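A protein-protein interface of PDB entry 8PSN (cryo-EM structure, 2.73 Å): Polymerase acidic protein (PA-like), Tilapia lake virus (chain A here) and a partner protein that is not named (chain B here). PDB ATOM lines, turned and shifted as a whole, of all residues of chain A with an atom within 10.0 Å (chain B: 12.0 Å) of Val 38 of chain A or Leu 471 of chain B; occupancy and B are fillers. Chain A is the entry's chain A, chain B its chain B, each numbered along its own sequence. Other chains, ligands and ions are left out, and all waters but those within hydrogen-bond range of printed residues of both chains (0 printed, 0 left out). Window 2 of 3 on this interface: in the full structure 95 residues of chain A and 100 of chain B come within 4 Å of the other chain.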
ATOM      1  N   MET A   1      -0.758  -6.121  18.571  1.00  0.00           N
ATOM      2  CA  MET A   1      -2.181  -6.523  18.753  1.00  0.00           C
ATOM      3  C   MET A   1      -2.873  -6.638  17.401  1.00  0.00           C
ATOM      4  O   MET A   1      -3.060  -5.640  16.704  1.00  0.00           O
ATOM      5  CB  MET A   1      -2.915  -5.516  19.636  1.00  0.00           C
ATOM      6  CG  MET A   1      -3.817  -6.150  20.678  1.00  0.00           C
ATOM      7  SD  MET A   1      -4.766  -4.929  21.600  1.00  0.00           S
ATOM      8  CE  MET A   1      -6.270  -5.846  21.922  1.00  0.00           C
ATOM      9  N   LEU A  26      -5.929 -13.853  30.925  1.00  0.00           N
ATOM     10  CA  LEU A  26      -6.810 -12.760  30.534  1.00  0.00           C
ATOM     11  C   LEU A  26      -6.504 -12.385  29.093  1.00  0.00           C
ATOM     12  O   LEU A  26      -5.366 -12.031  28.771  1.00  0.00           O
ATOM     13  CB  LEU A  26      -6.621 -11.554  31.453  1.00  0.00           C
ATOM     14  CG  LEU A  26      -6.792 -11.813  32.950  1.00  0.00           C
ATOM     15  CD1 LEU A  26      -6.551 -10.535  33.736  1.00  0.00           C
ATOM     16  CD2 LEU A  26      -8.172 -12.376  33.247  1.00  0.00           C
ATOM     17  N   SER A  27      -7.516 -12.462  28.232  1.00  0.00           N
ATOM     18  CA  SER A  27      -7.333 -12.172  26.817  1.00  0.00           C
ATOM     19  C   SER A  27      -7.414 -10.672  26.573  1.00  0.00           C
ATOM     20  O   SER A  27      -8.324 -10.001  27.069  1.00  0.00           O
ATOM     21  CB  SER A  27      -8.386 -12.902  25.984  1.00  0.00           C
ATOM     22  OG  SER A  27      -8.290 -12.545  24.617  1.00  0.00           O
ATOM     23  N   SER A  28      -6.457 -10.145  25.807  1.00  0.00           N
ATOM     24  CA  SER A  28      -6.454  -8.728  25.472  1.00  0.00           C
ATOM     25  C   SER A  28      -7.504  -8.367  24.433  1.00  0.00           C
ATOM     26  O   SER A  28      -7.744  -7.176  24.209  1.00  0.00           O
ATOM     27  CB  SER A  28      -5.071  -8.314  24.966  1.00  0.00           C
ATOM     28  OG  SER A  28      -4.104  -8.401  25.997  1.00  0.00           O
ATOM     29  N   SER A  30     -10.697  -9.407  24.697  1.00  0.00           N
ATOM     30  CA  SER A  30     -11.987  -9.507  25.365  1.00  0.00           C
ATOM     31  C   SER A  30     -12.216  -8.260  26.208  1.00  0.00           C
ATOM     32  O   SER A  30     -11.339  -7.856  26.977  1.00  0.00           O
ATOM     33  CB  SER A  30     -12.053 -10.757  26.243  1.00  0.00           C
ATOM     34  OG  SER A  30     -13.395 -11.098  26.545  1.00  0.00           O
ATOM     35  N   THR A  31     -13.396  -7.658  26.062  1.00  0.00           N
ATOM     36  CA  THR A  31     -13.722  -6.437  26.785  1.00  0.00           C
ATOM     37  C   THR A  31     -14.040  -6.681  28.254  1.00  0.00           C
ATOM     38  O   THR A  31     -14.156  -5.712  29.012  1.00  0.00           O
ATOM     39  CB  THR A  31     -14.909  -5.733  26.121  1.00  0.00           C
ATOM     40  OG1 THR A  31     -14.755  -5.766  24.696  1.00  0.00           O
ATOM     41  CG2 THR A  31     -15.004  -4.288  26.586  1.00  0.00           C
ATOM     42  N   GLU A  33     -12.420  -9.634  30.037  1.00  0.00           N
ATOM     43  CA  GLU A  33     -11.224 -10.207  30.639  1.00  0.00           C
ATOM     44  C   GLU A  33     -10.078  -9.208  30.717  1.00  0.00           C
ATOM     45  O   GLU A  33      -9.121  -9.441  31.461  1.00  0.00           O
ATOM     46  CB  GLU A  33     -10.771 -11.435  29.847  1.00  0.00           C
ATOM     47  CG  GLU A  33     -11.821 -12.528  29.741  1.00  0.00           C
ATOM     48  CD  GLU A  33     -12.346 -12.973  31.091  1.00  0.00           C
ATOM     49  OE1 GLU A  33     -11.544 -13.048  32.046  1.00  0.00           O
ATOM     50  OE2 GLU A  33     -13.559 -13.247  31.199  1.00  0.00           O
ATOM     51  N   ARG A  34     -10.156  -8.106  29.976  1.00  0.00           N
ATOM     52  CA  ARG A  34      -9.102  -7.104  30.009  1.00  0.00           C
ATOM     53  C   ARG A  34      -9.052  -6.428  31.372  1.00  0.00           C
ATOM     54  O   ARG A  34     -10.087  -6.132  31.975  1.00  0.00           O
ATOM     55  CB  ARG A  34      -9.329  -6.057  28.920  1.00  0.00           C
ATOM     56  CG  ARG A  34      -8.522  -6.284  27.658  1.00  0.00           C
ATOM     57  CD  ARG A  34      -8.878  -5.262  26.592  1.00  0.00           C
ATOM     58  NE  ARG A  34      -8.287  -3.957  26.871  1.00  0.00           N
ATOM     59  CZ  ARG A  34      -7.416  -3.330  26.089  1.00  0.00           C
ATOM     60  NH1 ARG A  34      -6.995  -3.857  24.951  1.00  0.00           N
ATOM     61  NH2 ARG A  34      -6.953  -2.140  26.461  1.00  0.00           N
ATOM     62  N   ARG A  35      -7.841  -6.184  31.857  1.00  0.00           N
ATOM     63  CA  ARG A  35      -7.665  -5.460  33.108  1.00  0.00           C
ATOM     64  C   ARG A  35      -7.874  -3.970  32.865  1.00  0.00           C
ATOM     65  O   ARG A  35      -7.158  -3.382  32.046  1.00  0.00           O
ATOM     66  CB  ARG A  35      -6.276  -5.706  33.680  1.00  0.00           C
ATOM     67  CG  ARG A  35      -6.205  -6.866  34.659  1.00  0.00           C
ATOM     68  CD  ARG A  35      -4.800  -7.046  35.211  1.00  0.00           C
ATOM     69  NE  ARG A  35      -3.807  -7.172  34.150  1.00  0.00           N
ATOM     70  CZ  ARG A  35      -2.565  -6.708  34.212  1.00  0.00           C
ATOM     71  NH1 ARG A  35      -2.112  -6.077  35.284  1.00  0.00           N
ATOM     72  NH2 ARG A  35      -1.756  -6.883  33.171  1.00  0.00           N
ATOM     73  N   PRO A  36      -8.826  -3.323  33.537  1.00  0.00           N
ATOM     74  CA  PRO A  36      -9.054  -1.897  33.285  1.00  0.00           C
ATOM     75  C   PRO A  36      -7.859  -1.052  33.695  1.00  0.00           C
ATOM     76  O   PRO A  36      -7.173  -1.335  34.679  1.00  0.00           O
ATOM     77  CB  PRO A  36     -10.284  -1.577  34.142  1.00  0.00           C
ATOM     78  CG  PRO A  36     -10.245  -2.576  35.237  1.00  0.00           C
ATOM     79  CD  PRO A  36      -9.673  -3.828  34.633  1.00  0.00           C
ATOM     80  N   GLY A  37      -7.625   0.007  32.926  1.00  0.00           N
ATOM     81  CA  GLY A  37      -6.528   0.913  33.226  1.00  0.00           C
ATOM     82  C   GLY A  37      -5.163   0.261  33.172  1.00  0.00           C
ATOM     83  O   GLY A  37      -4.302   0.563  34.007  1.00  0.00           O
ATOM     84  N   VAL A  38      -4.946  -0.631  32.209  1.00  0.00           N
ATOM     85  CA  VAL A  38      -3.657  -1.300  32.045  1.00  0.00           C
ATOM     86  C   VAL A  38      -3.358  -1.451  30.558  1.00  0.00           C
ATOM     87  O   VAL A  38      -4.098  -2.149  29.851  1.00  0.00           O
ATOM     88  CB  VAL A  38      -3.641  -2.669  32.743  1.00  0.00           C
ATOM     89  CG1 VAL A  38      -2.251  -3.284  32.674  1.00  0.00           C
ATOM     90  CG2 VAL A  38      -4.095  -2.542  34.187  1.00  0.00           C
ATOM     91  N   PRO A  39      -2.301  -0.827  30.036  1.00  0.00           N
ATOM     92  CA  PRO A  39      -1.932  -1.069  28.637  1.00  0.00           C
ATOM     93  C   PRO A  39      -1.594  -2.533  28.403  1.00  0.00           C
ATOM     94  O   PRO A  39      -1.053  -3.217  29.274  1.00  0.00           O
ATOM     95  CB  PRO A  39      -0.709  -0.169  28.428  1.00  0.00           C
ATOM     96  CG  PRO A  39      -0.822   0.876  29.475  1.00  0.00           C
ATOM     97  CD  PRO A  39      -1.458   0.211  30.653  1.00  0.00           C
ATOM     98  N   VAL A  40      -1.920  -3.011  27.207  1.00  0.00           N
ATOM     99  CA  VAL A  40      -1.699  -4.405  26.843  1.00  0.00           C
ATOM    100  C   VAL A  40      -0.328  -4.536  26.198  1.00  0.00           C
ATOM    101  O   VAL A  40       0.037  -3.748  25.318  1.00  0.00           O
ATOM    102  CB  VAL A  40      -2.805  -4.912  25.902  1.00  0.00           C
ATOM    103  CG1 VAL A  40      -4.175  -4.622  26.492  1.00  0.00           C
ATOM    104  CG2 VAL A  40      -2.667  -4.288  24.524  1.00  0.00           C
ATOM    105  N   GLU A  41       0.438  -5.528  26.647  1.00  0.00           N
ATOM    106  CA  GLU A  41       1.765  -5.802  26.117  1.00  0.00           C
ATOM    107  C   GLU A  41       1.849  -7.144  25.406  1.00  0.00           C
ATOM    108  O   GLU A  41       2.929  -7.512  24.932  1.00  0.00           O
ATOM    109  CB  GLU A  41       2.800  -5.751  27.245  1.00  0.00           C
ATOM    110  CG  GLU A  41       2.981  -4.373  27.856  1.00  0.00           C
ATOM    111  CD  GLU A  41       3.494  -4.429  29.279  1.00  0.00           C
ATOM    112  OE1 GLU A  41       4.451  -5.189  29.539  1.00  0.00           O
ATOM    113  OE2 GLU A  41       2.943  -3.713  30.140  1.00  0.00           O
ATOM    114  N   GLY A  42       0.748  -7.885  25.320  1.00  0.00           N
ATOM    115  CA  GLY A  42       0.749  -9.165  24.641  1.00  0.00           C
ATOM    116  C   GLY A  42      -0.665  -9.582  24.304  1.00  0.00           C
ATOM    117  O   GLY A  42      -1.634  -8.880  24.600  1.00  0.00           O
ATOM    118  N   TYR A  45      -2.523 -12.351  29.170  1.00  0.00           N
ATOM    119  CA  TYR A  45      -1.783 -12.041  30.388  1.00  0.00           C
ATOM    120  C   TYR A  45      -2.016 -13.151  31.400  1.00  0.00           C
ATOM    121  O   TYR A  45      -3.166 -13.474  31.715  1.00  0.00           O
ATOM    122  CB  TYR A  45      -2.221 -10.689  30.957  1.00  0.00           C
ATOM    123  CG  TYR A  45      -1.695 -10.390  32.342  1.00  0.00           C
ATOM    124  CD1 TYR A  45      -0.351 -10.120  32.550  1.00  0.00           C
ATOM    125  CD2 TYR A  45      -2.545 -10.371  33.438  1.00  0.00           C
ATOM    126  CE1 TYR A  45       0.133  -9.843  33.813  1.00  0.00           C
ATOM    127  CE2 TYR A  45      -2.071 -10.095  34.703  1.00  0.00           C
ATOM    128  CZ  TYR A  45      -0.732  -9.832  34.886  1.00  0.00           C
ATOM    129  OH  TYR A  45      -0.256  -9.557  36.146  1.00  0.00           O
ATOM    130  N   ASN A  50       2.113 -13.392  36.303  1.00  0.00           N
ATOM    131  CA  ASN A  50       2.165 -11.968  35.985  1.00  0.00           C
ATOM    132  C   ASN A  50       3.080 -11.713  34.788  1.00  0.00           C
ATOM    133  O   ASN A  50       4.076 -10.991  34.874  1.00  0.00           O
ATOM    134  CB  ASN A  50       2.622 -11.161  37.202  1.00  0.00           C
ATOM    135  CG  ASN A  50       1.643 -11.240  38.355  1.00  0.00           C
ATOM    136  OD1 ASN A  50       0.488 -10.831  38.234  1.00  0.00           O
ATOM    137  ND2 ASN A  50       2.101 -11.769  39.484  1.00  0.00           N
ATOM    138  N   TRP A  52       3.023 -11.298  30.272  1.00  0.00           N
ATOM    139  CA  TRP A  52       2.306 -11.223  29.008  1.00  0.00           C
ATOM    140  C   TRP A  52       2.808 -12.294  28.048  1.00  0.00           C
ATOM    141  O   TRP A  52       3.998 -12.618  28.021  1.00  0.00           O
ATOM    142  CB  TRP A  52       2.473  -9.840  28.385  1.00  0.00           C
ATOM    143  CG  TRP A  52       1.822  -8.754  29.177  1.00  0.00           C
ATOM    144  CD1 TRP A  52       2.396  -7.995  30.153  1.00  0.00           C
ATOM    145  CD2 TRP A  52       0.466  -8.306  29.066  1.00  0.00           C
ATOM    146  NE1 TRP A  52       1.484  -7.100  30.656  1.00  0.00           N
ATOM    147  CE2 TRP A  52       0.291  -7.271  30.004  1.00  0.00           C
ATOM    148  CE3 TRP A  52      -0.616  -8.678  28.263  1.00  0.00           C
ATOM    149  CZ2 TRP A  52      -0.920  -6.604  30.161  1.00  0.00           C
ATOM    150  CZ3 TRP A  52      -1.817  -8.015  28.421  1.00  0.00           C
ATOM    151  CH2 TRP A  52      -1.961  -6.992  29.364  1.00  0.00           C
ATOM    152  N   SER B 466     -22.396   3.713  26.814  1.00  0.00           N
ATOM    153  CA  SER B 466     -21.677   4.948  27.084  1.00  0.00           C
ATOM    154  C   SER B 466     -20.692   4.767  28.236  1.00  0.00           C
ATOM    155  O   SER B 466     -20.675   3.746  28.926  1.00  0.00           O
ATOM    156  CB  SER B 466     -22.663   6.075  27.405  1.00  0.00           C
ATOM    157  OG  SER B 466     -23.895   5.880  26.733  1.00  0.00           O
ATOM    158  N   ASP B 467     -19.860   5.790  28.434  1.00  0.00           N
ATOM    159  CA  ASP B 467     -18.932   5.854  29.561  1.00  0.00           C
ATOM    160  C   ASP B 467     -18.004   4.638  29.574  1.00  0.00           C
ATOM    161  O   ASP B 467     -18.017   3.815  30.491  1.00  0.00           O
ATOM    162  CB  ASP B 467     -19.702   5.980  30.879  1.00  0.00           C
ATOM    163  CG  ASP B 467     -18.838   6.477  32.017  1.00  0.00           C
ATOM    164  OD1 ASP B 467     -18.097   7.463  31.821  1.00  0.00           O
ATOM    165  OD2 ASP B 467     -18.903   5.885  33.112  1.00  0.00           O
ATOM    166  N   LEU B 468     -17.191   4.542  28.529  1.00  0.00           N
ATOM    167  CA  LEU B 468     -16.294   3.415  28.330  1.00  0.00           C
ATOM    168  C   LEU B 468     -14.878   3.755  28.776  1.00  0.00           C
ATOM    169  O   LEU B 468     -14.490   4.921  28.878  1.00  0.00           O
ATOM    170  CB  LEU B 468     -16.284   2.989  26.859  1.00  0.00           C
ATOM    171  CG  LEU B 468     -16.904   1.626  26.551  1.00  0.00           C
ATOM    172  CD1 LEU B 468     -18.355   1.562  27.005  1.00  0.00           C
ATOM    173  CD2 LEU B 468     -16.794   1.329  25.067  1.00  0.00           C
ATOM    174  N   ASP B 469     -14.107   2.708  29.039  1.00  0.00           N
ATOM    175  CA  ASP B 469     -12.713   2.879  29.417  1.00  0.00           C
ATOM    176  C   ASP B 469     -11.949   3.528  28.265  1.00  0.00           C
ATOM    177  O   ASP B 469     -12.070   3.076  27.118  1.00  0.00           O
ATOM    178  CB  ASP B 469     -12.098   1.526  29.769  1.00  0.00           C
ATOM    179  CG  ASP B 469     -10.704   1.645  30.347  1.00  0.00           C
ATOM    180  OD1 ASP B 469     -10.461   2.575  31.142  1.00  0.00           O
ATOM    181  OD2 ASP B 469      -9.850   0.798  30.012  1.00  0.00           O
ATOM    182  N   PRO B 470     -11.162   4.579  28.513  1.00  0.00           N
ATOM    183  CA  PRO B 470     -10.439   5.221  27.405  1.00  0.00           C
ATOM    184  C   PRO B 470      -9.370   4.339  26.776  1.00  0.00           C
ATOM    185  O   PRO B 470      -8.775   4.721  25.764  1.00  0.00           O
ATOM    186  CB  PRO B 470      -9.817   6.462  28.060  1.00  0.00           C
ATOM    187  CG  PRO B 470      -9.847   6.200  29.520  1.00  0.00           C
ATOM    188  CD  PRO B 470     -11.043   5.352  29.760  1.00  0.00           C
ATOM    189  N   LEU B 471      -9.111   3.165  27.353  1.00  0.00           N
ATOM    190  CA  LEU B 471      -8.069   2.279  26.849  1.00  0.00           C
ATOM    191  C   LEU B 471      -8.593   1.174  25.944  1.00  0.00           C
ATOM    192  O   LEU B 471      -7.877   0.757  25.028  1.00  0.00           O
ATOM    193  CB  LEU B 471      -7.308   1.636  28.013  1.00  0.00           C
ATOM    194  CG  LEU B 471      -6.340   2.534  28.786  1.00  0.00           C
ATOM    195  CD1 LEU B 471      -5.777   1.785  29.979  1.00  0.00           C
ATOM    196  CD2 LEU B 471      -5.218   3.028  27.889  1.00  0.00           C
ATOM    197  N   VAL B 472      -9.809   0.687  26.167  1.00  0.00           N
ATOM    198  CA  VAL B 472     -10.335  -0.427  25.382  1.00  0.00           C
ATOM    199  C   VAL B 472     -10.533   0.048  23.946  1.00  0.00           C
ATOM    200  O   VAL B 472     -11.256   1.028  23.718  1.00  0.00           O
ATOM    201  CB  VAL B 472     -11.645  -0.970  25.978  1.00  0.00           C
ATOM    202  CG1 VAL B 472     -12.734   0.092  25.963  1.00  0.00           C
ATOM    203  CG2 VAL B 472     -12.098  -2.218  25.233  1.00  0.00           C
ATOM    204  N   PRO B 473      -9.920  -0.593  22.952  1.00  0.00           N
ATOM    205  CA  PRO B 473     -10.168  -0.187  21.565  1.00  0.00           C
ATOM    206  C   PRO B 473     -11.604  -0.466  21.157  1.00  0.00           C
ATOM    207  O   PRO B 473     -12.242  -1.405  21.637  1.00  0.00           O
ATOM    208  CB  PRO B 473      -9.183  -1.036  20.750  1.00  0.00           C
ATOM    209  CG  PRO B 473      -8.258  -1.659  21.733  1.00  0.00           C
ATOM    210  CD  PRO B 473      -8.976  -1.720  23.033  1.00  0.00           C
ATOM    211  N   HIS B 474     -12.111   0.369  20.252  1.00  0.00           N
ATOM    212  CA  HIS B 474     -13.480   0.222  19.775  1.00  0.00           C
ATOM    213  C   HIS B 474     -13.633  -0.886  18.742  1.00  0.00           C
ATOM    214  O   HIS B 474     -14.765  -1.205  18.366  1.00  0.00           O
ATOM    215  CB  HIS B 474     -13.974   1.543  19.184  1.00  0.00           C
ATOM    216  CG  HIS B 474     -14.232   2.604  20.208  1.00  0.00           C
ATOM    217  ND1 HIS B 474     -14.076   3.947  19.944  1.00  0.00           N
ATOM    218  CD2 HIS B 474     -14.637   2.520  21.497  1.00  0.00           C
ATOM    219  CE1 HIS B 474     -14.372   4.645  21.025  1.00  0.00           C
ATOM    220  NE2 HIS B 474     -14.716   3.802  21.982  1.00  0.00           N
ATOM    221  N   ARG B 475     -12.534  -1.475  18.275  1.00  0.00           N
ATOM    222  CA  ARG B 475     -12.603  -2.571  17.318  1.00  0.00           C
ATOM    223  C   ARG B 475     -12.839  -3.922  17.982  1.00  0.00           C
ATOM    224  O   ARG B 475     -12.984  -4.922  17.273  1.00  0.00           O
ATOM    225  CB  ARG B 475     -11.316  -2.623  16.489  1.00  0.00           C
ATOM    226  CG  ARG B 475     -10.075  -2.981  17.290  1.00  0.00           C
ATOM    227  CD  ARG B 475      -8.864  -2.194  16.818  1.00  0.00           C
ATOM    228  NE  ARG B 475      -7.624  -2.702  17.398  1.00  0.00           N
ATOM    229  CZ  ARG B 475      -6.649  -1.951  17.894  1.00  0.00           C
ATOM    230  NH1 ARG B 475      -6.718  -0.629  17.893  1.00  0.00           N
ATOM    231  NH2 ARG B 475      -5.571  -2.541  18.402  1.00  0.00           N
ATOM    232  N   LEU B 476     -12.882  -3.977  19.310  1.00  0.00           N
ATOM    233  CA  LEU B 476     -13.130  -5.230  20.007  1.00  0.00           C
ATOM    234  C   LEU B 476     -14.599  -5.619  19.902  1.00  0.00           C
ATOM    235  O   LEU B 476     -15.482  -4.772  19.747  1.00  0.00           O
ATOM    236  CB  LEU B 476     -12.724  -5.118  21.476  1.00  0.00           C
ATOM    237  CG  LEU B 476     -11.254  -4.796  21.760  1.00  0.00           C
ATOM    238  CD1 LEU B 476     -10.947  -5.023  23.228  1.00  0.00           C
ATOM    239  CD2 LEU B 476     -10.318  -5.619  20.884  1.00  0.00           C
ATOM    240  N   LEU B 477     -14.852  -6.922  19.998  1.00  0.00           N
ATOM    241  CA  LEU B 477     -16.186  -7.471  19.807  1.00  0.00           C
ATOM    242  C   LEU B 477     -16.871  -7.699  21.147  1.00  0.00           C
ATOM    243  O   LEU B 477     -16.255  -8.187  22.099  1.00  0.00           O
ATOM    244  CB  LEU B 477     -16.109  -8.789  19.036  1.00  0.00           C
ATOM    245  CG  LEU B 477     -15.484  -8.707  17.644  1.00  0.00           C
ATOM    246  CD1 LEU B 477     -15.291 -10.101  17.071  1.00  0.00           C
ATOM    247  CD2 LEU B 477     -16.339  -7.859  16.720  1.00  0.00           C
ATOM    248  N   VAL B 478     -18.154  -7.343  21.213  1.00  0.00           N
ATOM    249  CA  VAL B 478     -18.961  -7.527  22.411  1.00  0.00           C
ATOM    250  C   VAL B 478     -20.298  -8.147  22.026  1.00  0.00           C
ATOM    251  O   VAL B 478     -20.773  -8.016  20.897  1.00  0.00           O
ATOM    252  CB  VAL B 478     -19.189  -6.202  23.170  1.00  0.00           C
ATOM    253  CG1 VAL B 478     -17.866  -5.622  23.623  1.00  0.00           C
ATOM    254  CG2 VAL B 478     -19.938  -5.205  22.298  1.00  0.00           C
ATOM    255  N   ILE B 486     -20.476  -4.797  31.311  1.00  0.00           N
ATOM    256  CA  ILE B 486     -19.739  -3.534  31.316  1.00  0.00           C
ATOM    257  C   ILE B 486     -20.559  -2.451  32.004  1.00  0.00           C
ATOM    258  O   ILE B 486     -20.055  -1.706  32.857  1.00  0.00           O
ATOM    259  CB  ILE B 486     -19.366  -3.131  29.879  1.00  0.00           C
ATOM    260  CG1 ILE B 486     -18.203  -3.982  29.371  1.00  0.00           C
ATOM    261  CG2 ILE B 486     -18.998  -1.658  29.811  1.00  0.00           C
ATOM    262  CD1 ILE B 486     -18.136  -4.072  27.863  1.00  0.00           C
ATOM    263  N   ARG B 490     -19.603  -0.502  35.525  1.00  0.00           N
ATOM    264  CA  ARG B 490     -19.458   0.949  35.595  1.00  0.00           C
ATOM    265  C   ARG B 490     -20.435   1.552  36.597  1.00  0.00           C
ATOM    266  O   ARG B 490     -20.075   2.457  37.361  1.00  0.00           O
ATOM    267  CB  ARG B 490     -19.653   1.571  34.212  1.00  0.00           C
ATOM    268  CG  ARG B 490     -19.307   3.059  34.136  1.00  0.00           C
ATOM    269  CD  ARG B 490     -17.902   3.357  34.650  1.00  0.00           C
ATOM    270  NE  ARG B 490     -17.558   4.768  34.524  1.00  0.00           N
ATOM    271  CZ  ARG B 490     -16.467   5.319  35.038  1.00  0.00           C
ATOM    272  NH1 ARG B 490     -15.599   4.609  35.740  1.00  0.00           N
ATOM    273  NH2 ARG B 490     -16.242   6.615  34.844  1.00  0.00           N
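The guanidinium group of Arg 34 of chain A is in hydrogen-bond range of the backbone carbonyl oxygen of Leu 471 of chain B, 3.4 Å away.
The guanidinium group (NH1) of Arg 34 of chain A sits close to the backbone carbonyl oxygen (O) of Ser 28 of chain A (3.5 Å). O of Gly 42 of chain A is in hydrogen-bond range of OG of Ser 28 of chain A (2.9 Å).
Thr 31 of chain A touches Val 472 of chain B. Thr 31 of chain A touches Leu 476 of chain B. Thr 31 of chain A touches Val 478 of chain B. CD1 of Ile 486 of chain B touches CG2 of Thr 31 of chain A, 3.4 Å away. Arg 34 of chain A touches Val 472 of chain B (NH2 to CA, 3.9 Å). Arg 34 of chain A touches Pro 473 of chain B. Arg 34 of chain A touches Leu 476 of chain B. N of Gly 37 of chain A touches OD2 of Asp 469 of chain B, at 3.8 Å. CA of Gly 37 of chain A touches CD1 of Leu 471 of chain B, 3.4 Å away. Val 38 of chain A touches Leu 471 of chain B (N to CD1, 3.4 Å).
Of the printed residues of chain B, Ser 28 of chain A touches Leu 476 (3.98 Å). Of the printed residues of chain B, Arg 34 of chain A touches Leu 471, Val 472, Pro 473 and Leu 476. No residue of chain B comes within 4 Å of Arg 35 of chain A. No residue of chain B comes within 4 Å of Pro 36 of chain A. Gly 37 of chain A touches two residues of chain B. Pro 39 of chain A touches none of the printed residues of chain B. No residue of chain B comes within 4 Å of Val 40 of chain A. Gly 42 of chain A touches none of the printed residues of chain B. No residue of chain A comes within 4 Å of Pro 470 of chain B. Of chain A, only Thr 31 (3.8 Å) and Arg 34 (3.9 Å) come within 4 Å of Val 472 of chain B. Of chain A, only Arg 34 comes within 4 Å of Pro 473 of chain B. The nearest residue of chain A that does not touch Leu 471 of chain B is Pro 39 of chain A (4.3 Å). The nearest printed residue of chain B that does not touch Arg 34 of chain A is Asp 469 of chain B (5.4 Å).
Of the 15 printed residues of chain B, 8 touch a printed residue of chain A. Printed residues of chain B that touch a printed residue of chain A: Asp 469, Leu 471, Val 472, Pro 473, Leu 476, Leu 477, Val 478 and Ile 486. Hydrophobic or aromatic side chains of chain B within 4 Å of the printed part of chain A: Leu 471, Val 472, Pro 473, Leu 476, Val 478 and Ile 486. Of the 19 printed residues of chain A, 5 touch a printed residue of chain B. Along chain A the printed residues that touch a printed residue of chain B span positions 28 to 38.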
